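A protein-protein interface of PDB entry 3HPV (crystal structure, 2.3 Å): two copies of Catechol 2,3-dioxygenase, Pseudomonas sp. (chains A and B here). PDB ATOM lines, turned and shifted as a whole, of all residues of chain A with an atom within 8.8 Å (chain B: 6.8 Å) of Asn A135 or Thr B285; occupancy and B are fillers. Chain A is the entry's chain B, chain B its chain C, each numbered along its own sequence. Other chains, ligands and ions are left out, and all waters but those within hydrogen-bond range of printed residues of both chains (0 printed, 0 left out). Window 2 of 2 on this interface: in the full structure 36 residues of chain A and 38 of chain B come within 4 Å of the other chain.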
ATOM      1  N   ILE A 131      -1.337 -29.334 -26.887  1.00  0.00           N
ATOM      2  CA  ILE A 131      -0.467 -28.555 -25.996  1.00  0.00           C
ATOM      3  C   ILE A 131       0.878 -29.292 -25.853  1.00  0.00           C
ATOM      4  O   ILE A 131       0.920 -30.525 -25.933  1.00  0.00           O
ATOM      5  CB  ILE A 131      -1.087 -28.395 -24.575  1.00  0.00           C
ATOM      6  CG1 ILE A 131      -2.437 -27.687 -24.650  1.00  0.00           C
ATOM      7  CG2 ILE A 131      -0.150 -27.603 -23.693  1.00  0.00           C
ATOM      8  CD1 ILE A 131      -3.130 -27.575 -23.310  1.00  0.00           C
ATOM      9  N   SER A 132       1.965 -28.554 -25.624  1.00  0.00           N
ATOM     10  CA  SER A 132       3.288 -29.167 -25.493  1.00  0.00           C
ATOM     11  C   SER A 132       3.463 -30.129 -24.308  1.00  0.00           C
ATOM     12  O   SER A 132       2.751 -30.062 -23.306  1.00  0.00           O
ATOM     13  CB  SER A 132       4.363 -28.085 -25.430  1.00  0.00           C
ATOM     14  OG  SER A 132       4.294 -27.370 -24.218  1.00  0.00           O
ATOM     15  N   GLU A 133       4.431 -31.026 -24.437  1.00  0.00           N
ATOM     16  CA  GLU A 133       4.714 -32.026 -23.416  1.00  0.00           C
ATOM     17  C   GLU A 133       5.595 -31.419 -22.321  1.00  0.00           C
ATOM     18  O   GLU A 133       5.706 -31.955 -21.210  1.00  0.00           O
ATOM     19  CB  GLU A 133       5.426 -33.229 -24.065  1.00  0.00           C
ATOM     20  CG  GLU A 133       5.631 -34.426 -23.151  1.00  0.00           C
ATOM     21  CD  GLU A 133       4.699 -35.598 -23.482  1.00  0.00           C
ATOM     22  OE1 GLU A 133       3.483 -35.372 -23.697  1.00  0.00           O
ATOM     23  OE2 GLU A 133       5.187 -36.751 -23.517  1.00  0.00           O
ATOM     24  N   VAL A 134       6.222 -30.295 -22.644  1.00  0.00           N
ATOM     25  CA  VAL A 134       7.096 -29.614 -21.706  1.00  0.00           C
ATOM     26  C   VAL A 134       6.540 -28.234 -21.375  1.00  0.00           C
ATOM     27  O   VAL A 134       6.180 -27.469 -22.272  1.00  0.00           O
ATOM     28  CB  VAL A 134       8.511 -29.483 -22.293  1.00  0.00           C
ATOM     29  CG1 VAL A 134       8.426 -28.971 -23.734  1.00  0.00           C
ATOM     30  CG2 VAL A 134       9.350 -28.559 -21.428  1.00  0.00           C
ATOM     31  N   ASN A 135       6.481 -27.929 -20.079  1.00  0.00           N
ATOM     32  CA  ASN A 135       5.955 -26.656 -19.581  1.00  0.00           C
ATOM     33  C   ASN A 135       4.615 -26.322 -20.257  1.00  0.00           C
ATOM     34  O   ASN A 135       4.413 -25.218 -20.755  1.00  0.00           O
ATOM     35  CB  ASN A 135       6.977 -25.529 -19.826  1.00  0.00           C
ATOM     36  CG  ASN A 135       8.273 -25.727 -19.048  1.00  0.00           C
ATOM     37  OD1 ASN A 135       8.263 -25.931 -17.835  1.00  0.00           O
ATOM     38  ND2 ASN A 135       9.391 -25.659 -19.748  1.00  0.00           N
ATOM     39  N   PRO A 136       3.671 -27.277 -20.257  1.00  0.00           N
ATOM     40  CA  PRO A 136       2.361 -27.082 -20.881  1.00  0.00           C
ATOM     41  C   PRO A 136       1.487 -26.010 -20.261  1.00  0.00           C
ATOM     42  O   PRO A 136       1.398 -25.903 -19.040  1.00  0.00           O
ATOM     43  CB  PRO A 136       1.719 -28.457 -20.744  1.00  0.00           C
ATOM     44  CG  PRO A 136       2.223 -28.898 -19.427  1.00  0.00           C
ATOM     45  CD  PRO A 136       3.687 -28.536 -19.487  1.00  0.00           C
ATOM     46  N   ALA A 137       0.836 -25.222 -21.104  1.00  0.00           N
ATOM     47  CA  ALA A 137      -0.092 -24.209 -20.616  1.00  0.00           C
ATOM     48  C   ALA A 137      -1.318 -25.033 -20.217  1.00  0.00           C
ATOM     49  O   ALA A 137      -1.436 -26.196 -20.624  1.00  0.00           O
ATOM     50  CB  ALA A 137      -0.451 -23.235 -21.729  1.00  0.00           C
ATOM     51  N   PRO A 138      -2.239 -24.450 -19.421  1.00  0.00           N
ATOM     52  CA  PRO A 138      -3.463 -25.135 -18.960  1.00  0.00           C
ATOM     53  C   PRO A 138      -4.530 -25.407 -20.045  1.00  0.00           C
ATOM     54  O   PRO A 138      -5.436 -26.233 -19.851  1.00  0.00           O
ATOM     55  CB  PRO A 138      -3.958 -24.224 -17.833  1.00  0.00           C
ATOM     56  CG  PRO A 138      -3.529 -22.857 -18.304  1.00  0.00           C
ATOM     57  CD  PRO A 138      -2.130 -23.101 -18.831  1.00  0.00           C
ATOM     58  N   ARG B 180       6.481 -34.250 -13.866  1.00  0.00           N
ATOM     59  CA  ARG B 180       7.744 -34.159 -13.147  1.00  0.00           C
ATOM     60  C   ARG B 180       8.306 -32.772 -13.300  1.00  0.00           C
ATOM     61  O   ARG B 180       7.941 -32.034 -14.216  1.00  0.00           O
ATOM     62  CB  ARG B 180       8.782 -35.153 -13.675  1.00  0.00           C
ATOM     63  CG  ARG B 180       9.434 -34.728 -14.978  1.00  0.00           C
ATOM     64  CD  ARG B 180       8.766 -35.384 -16.162  1.00  0.00           C
ATOM     65  NE  ARG B 180       9.608 -36.419 -16.767  1.00  0.00           N
ATOM     66  CZ  ARG B 180      10.153 -37.438 -16.106  1.00  0.00           C
ATOM     67  NH1 ARG B 180       9.961 -37.577 -14.804  1.00  0.00           N
ATOM     68  NH2 ARG B 180      10.876 -38.333 -16.759  1.00  0.00           N
ATOM     69  N   VAL B 181       9.187 -32.419 -12.377  1.00  0.00           N
ATOM     70  CA  VAL B 181       9.876 -31.142 -12.423  1.00  0.00           C
ATOM     71  C   VAL B 181      11.356 -31.499 -12.524  1.00  0.00           C
ATOM     72  O   VAL B 181      11.919 -32.165 -11.648  1.00  0.00           O
ATOM     73  CB  VAL B 181       9.650 -30.295 -11.163  1.00  0.00           C
ATOM     74  CG1 VAL B 181      10.500 -29.038 -11.241  1.00  0.00           C
ATOM     75  CG2 VAL B 181       8.190 -29.930 -11.041  1.00  0.00           C
ATOM     76  N   LEU B 182      11.968 -31.073 -13.622  1.00  0.00           N
ATOM     77  CA  LEU B 182      13.376 -31.324 -13.868  1.00  0.00           C
ATOM     78  C   LEU B 182      14.265 -30.600 -12.877  1.00  0.00           C
ATOM     79  O   LEU B 182      13.811 -29.766 -12.093  1.00  0.00           O
ATOM     80  CB  LEU B 182      13.728 -30.892 -15.294  1.00  0.00           C
ATOM     81  CG  LEU B 182      13.563 -31.974 -16.369  1.00  0.00           C
ATOM     82  CD1 LEU B 182      12.365 -32.852 -16.069  1.00  0.00           C
ATOM     83  CD2 LEU B 182      13.445 -31.326 -17.732  1.00  0.00           C
ATOM     84  N   SER B 183      15.538 -30.960 -12.894  1.00  0.00           N
ATOM     85  CA  SER B 183      16.523 -30.317 -12.046  1.00  0.00           C
ATOM     86  C   SER B 183      17.218 -29.396 -13.041  1.00  0.00           C
ATOM     87  O   SER B 183      17.101 -29.594 -14.253  1.00  0.00           O
ATOM     88  CB  SER B 183      17.497 -31.353 -11.466  1.00  0.00           C
ATOM     89  OG  SER B 183      18.027 -32.196 -12.477  1.00  0.00           O
ATOM     90  N   PRO B 184      17.933 -28.372 -12.555  1.00  0.00           N
ATOM     91  CA  PRO B 184      18.614 -27.465 -13.487  1.00  0.00           C
ATOM     92  C   PRO B 184      19.292 -28.217 -14.633  1.00  0.00           C
ATOM     93  O   PRO B 184      19.057 -27.922 -15.806  1.00  0.00           O
ATOM     94  CB  PRO B 184      19.601 -26.725 -12.585  1.00  0.00           C
ATOM     95  CG  PRO B 184      19.820 -27.684 -11.448  1.00  0.00           C
ATOM     96  CD  PRO B 184      18.430 -28.174 -11.187  1.00  0.00           C
ATOM     97  N   LEU B 282       4.088 -35.426 -18.114  1.00  0.00           N
ATOM     98  CA  LEU B 282       4.354 -34.068 -18.615  1.00  0.00           C
ATOM     99  C   LEU B 282       5.606 -33.536 -17.920  1.00  0.00           C
ATOM    100  O   LEU B 282       5.877 -33.882 -16.778  1.00  0.00           O
ATOM    101  CB  LEU B 282       3.185 -33.119 -18.304  1.00  0.00           C
ATOM    102  CG  LEU B 282       1.829 -33.371 -18.961  1.00  0.00           C
ATOM    103  CD1 LEU B 282       0.852 -32.276 -18.559  1.00  0.00           C
ATOM    104  CD2 LEU B 282       1.988 -33.393 -20.456  1.00  0.00           C
ATOM    105  N   SER B 283       6.370 -32.688 -18.589  1.00  0.00           N
ATOM    106  CA  SER B 283       7.577 -32.180 -17.952  1.00  0.00           C
ATOM    107  C   SER B 283       7.691 -30.663 -17.846  1.00  0.00           C
ATOM    108  O   SER B 283       7.253 -29.926 -18.720  1.00  0.00           O
ATOM    109  CB  SER B 283       8.809 -32.736 -18.663  1.00  0.00           C
ATOM    110  OG  SER B 283       8.803 -34.151 -18.637  1.00  0.00           O
ATOM    111  N   TRP B 284       8.282 -30.216 -16.746  1.00  0.00           N
ATOM    112  CA  TRP B 284       8.503 -28.799 -16.501  1.00  0.00           C
ATOM    113  C   TRP B 284      10.009 -28.577 -16.303  1.00  0.00           C
ATOM    114  O   TRP B 284      10.657 -29.297 -15.531  1.00  0.00           O
ATOM    115  CB  TRP B 284       7.737 -28.338 -15.250  1.00  0.00           C
ATOM    116  CG  TRP B 284       6.233 -28.363 -15.396  1.00  0.00           C
ATOM    117  CD1 TRP B 284       5.411 -29.445 -15.244  1.00  0.00           C
ATOM    118  CD2 TRP B 284       5.387 -27.274 -15.800  1.00  0.00           C
ATOM    119  NE1 TRP B 284       4.110 -29.098 -15.535  1.00  0.00           N
ATOM    120  CE2 TRP B 284       4.069 -27.774 -15.881  1.00  0.00           C
ATOM    121  CE3 TRP B 284       5.616 -25.928 -16.101  1.00  0.00           C
ATOM    122  CZ2 TRP B 284       2.984 -26.973 -16.256  1.00  0.00           C
ATOM    123  CZ3 TRP B 284       4.529 -25.131 -16.471  1.00  0.00           C
ATOM    124  CH2 TRP B 284       3.232 -25.661 -16.547  1.00  0.00           C
ATOM    125  N   THR B 285      10.566 -27.604 -17.021  1.00  0.00           N
ATOM    126  CA  THR B 285      11.984 -27.294 -16.887  1.00  0.00           C
ATOM    127  C   THR B 285      12.166 -26.584 -15.549  1.00  0.00           C
ATOM    128  O   THR B 285      11.256 -25.901 -15.076  1.00  0.00           O
ATOM    129  CB  THR B 285      12.486 -26.385 -18.039  1.00  0.00           C
ATOM    130  OG1 THR B 285      11.579 -25.295 -18.230  1.00  0.00           O
ATOM    131  CG2 THR B 285      12.591 -27.174 -19.330  1.00  0.00           C
ATOM    132  N   TYR B 286      13.336 -26.748 -14.940  1.00  0.00           N
ATOM    133  CA  TYR B 286      13.621 -26.148 -13.639  1.00  0.00           C
ATOM    134  C   TYR B 286      13.346 -24.637 -13.525  1.00  0.00           C
ATOM    135  O   TYR B 286      12.979 -24.144 -12.458  1.00  0.00           O
ATOM    136  CB  TYR B 286      15.076 -26.426 -13.246  1.00  0.00           C
ATOM    137  CG  TYR B 286      15.309 -26.256 -11.771  1.00  0.00           C
ATOM    138  CD1 TYR B 286      14.839 -27.207 -10.870  1.00  0.00           C
ATOM    139  CD2 TYR B 286      15.934 -25.112 -11.263  1.00  0.00           C
ATOM    140  CE1 TYR B 286      14.979 -27.029  -9.498  1.00  0.00           C
ATOM    141  CE2 TYR B 286      16.077 -24.922  -9.885  1.00  0.00           C
ATOM    142  CZ  TYR B 286      15.593 -25.887  -9.012  1.00  0.00           C
ATOM    143  OH  TYR B 286      15.698 -25.721  -7.645  1.00  0.00           O
ATOM    144  N   ASP B 287      13.527 -23.901 -14.615  1.00  0.00           N
ATOM    145  CA  ASP B 287      13.289 -22.464 -14.585  1.00  0.00           C
ATOM    146  C   ASP B 287      11.852 -22.053 -14.216  1.00  0.00           C
ATOM    147  O   ASP B 287      11.662 -21.053 -13.518  1.00  0.00           O
ATOM    148  CB  ASP B 287      13.699 -21.837 -15.923  1.00  0.00           C
ATOM    149  CG  ASP B 287      13.292 -22.677 -17.116  1.00  0.00           C
ATOM    150  OD1 ASP B 287      12.079 -22.943 -17.273  1.00  0.00           O
ATOM    151  OD2 ASP B 287      14.183 -23.071 -17.901  1.00  0.00           O
ATOM    152  N   ASN B 288      10.845 -22.806 -14.661  1.00  0.00           N
ATOM    153  CA  ASN B 288       9.451 -22.473 -14.339  1.00  0.00           C
ATOM    154  C   ASN B 288       9.087 -22.822 -12.905  1.00  0.00           C
ATOM    155  O   ASN B 288       8.343 -22.086 -12.248  1.00  0.00           O
ATOM    156  CB  ASN B 288       8.483 -23.197 -15.275  1.00  0.00           C
ATOM    157  CG  ASN B 288       8.623 -22.749 -16.712  1.00  0.00           C
ATOM    158  OD1 ASN B 288       7.839 -23.144 -17.576  1.00  0.00           O
ATOM    159  ND2 ASN B 288       9.631 -21.919 -16.979  1.00  0.00           N
ATOM    160  N   PHE B 289       9.603 -23.955 -12.437  1.00  0.00           N
ATOM    161  CA  PHE B 289       9.357 -24.422 -11.081  1.00  0.00           C
ATOM    162  C   PHE B 289       9.832 -23.357 -10.110  1.00  0.00           C
ATOM    163  O   PHE B 289      10.796 -23.628  -9.371  1.00  0.00           O
ATOM    164  CB  PHE B 289      10.107 -25.739 -10.833  1.00  0.00           C
ATOM    165  CG  PHE B 289       9.911 -26.314  -9.448  1.00  0.00           C
ATOM    166  CD1 PHE B 289       8.636 -26.623  -8.974  1.00  0.00           C
ATOM    167  CD2 PHE B 289      11.007 -26.560  -8.620  1.00  0.00           C
ATOM    168  CE1 PHE B 289       8.459 -27.164  -7.699  1.00  0.00           C
ATOM    169  CE2 PHE B 289      10.839 -27.103  -7.343  1.00  0.00           C
ATOM    170  CZ  PHE B 289       9.564 -27.404  -6.881  1.00  0.00           C
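OG of Ser A132 sits at hydrogen-bond distance from O of Val A134, 2.7 Å away. O of Arg B180 sits at hydrogen-bond distance from N of Trp B284, at 3.1 Å. The side-chain hydroxyl (OG1) of Thr B285 lies within hydrogen-bond range of the side-chain carboxylate (OD1) of Asp B287, at 2.6 Å. The backbone NH (N) of Arg B180 lies within hydrogen-bond range of the backbone carbonyl oxygen (O) of Leu B282, 3.0 Å away. The side-chain carboxylate (OD1) of Asp B287 is in hydrogen-bond range of the side-chain amide nitrogen (ND2) of Asn B288, at 2.7 Å. N of Leu B182 sits at hydrogen-bond distance from O of Trp B284 (2.9 Å).
Asn A135 touches just these residues of chain B: Ser B283, Trp B284, Thr B285 and Asn B288. Printed residues of chain B within 4 Å of Pro A136: Leu B282, Ser B283 and Trp B284. Pro B184 touches none of the printed residues of chain A. Of the printed residues of chain A, Leu B282 touches Glu A133 (3.6 Å) and Pro A136 (3.7 Å). Of the printed residues of chain A, Ser B283 touches Glu A133, Val A134, Asn A135 and Pro A136. Printed residues of chain A within 4 Å of Trp B284: Asn A135 and Pro A136. Of chain A, only Asn A135 comes within 4 Å of Thr B285. Of the printed residues of chain A, Asn B288 touches Asn A135. The nearest printed residue of chain B that does not touch Val A134 is Thr B285 (4.1 Å).
No position is printed for both chains. Of the 10 pairs that touch across the chains among the printed residues, none has its exchanged pair printed and touching as well.
The side-chain amide nitrogen of Asn A135 sits at hydrogen-bond distance from the side-chain hydroxyl of Thr B285 (2.7 Å). OD1 of Asn A135 sits close to OD1 of Asn B288 (2.8 Å). The backbone NH (N) of Asn A135 lies within hydrogen-bond range of the backbone carbonyl oxygen (O) of Ser B283, at 2.5 Å. The backbone NH (N) of Ser B283 sits at hydrogen-bond distance from the backbone carbonyl oxygen (O) of Glu A133.
Among the printed residues, merely in contact across the chains: Val A134 with Ser B283, Pro A136 with Trp B284, Asn A135 with Trp B284, Glu A133 with Leu B282, Pro A136 with Leu B282 and Pro A136 with Ser B283.
Printed residues of chain B that touch a printed residue of chain A: Leu B282, Ser B283, Trp B284, Thr B285 and Asn B288. Of the 8 printed residues of chain A, 4 touch a printed residue of chain B. Among the printed residues, 10 pairs touch across the chains. Among the printed residues, no Asp or Glu carboxylate lies within 4 Å of a Lys or Arg side-chain nitrogen of the other chain.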
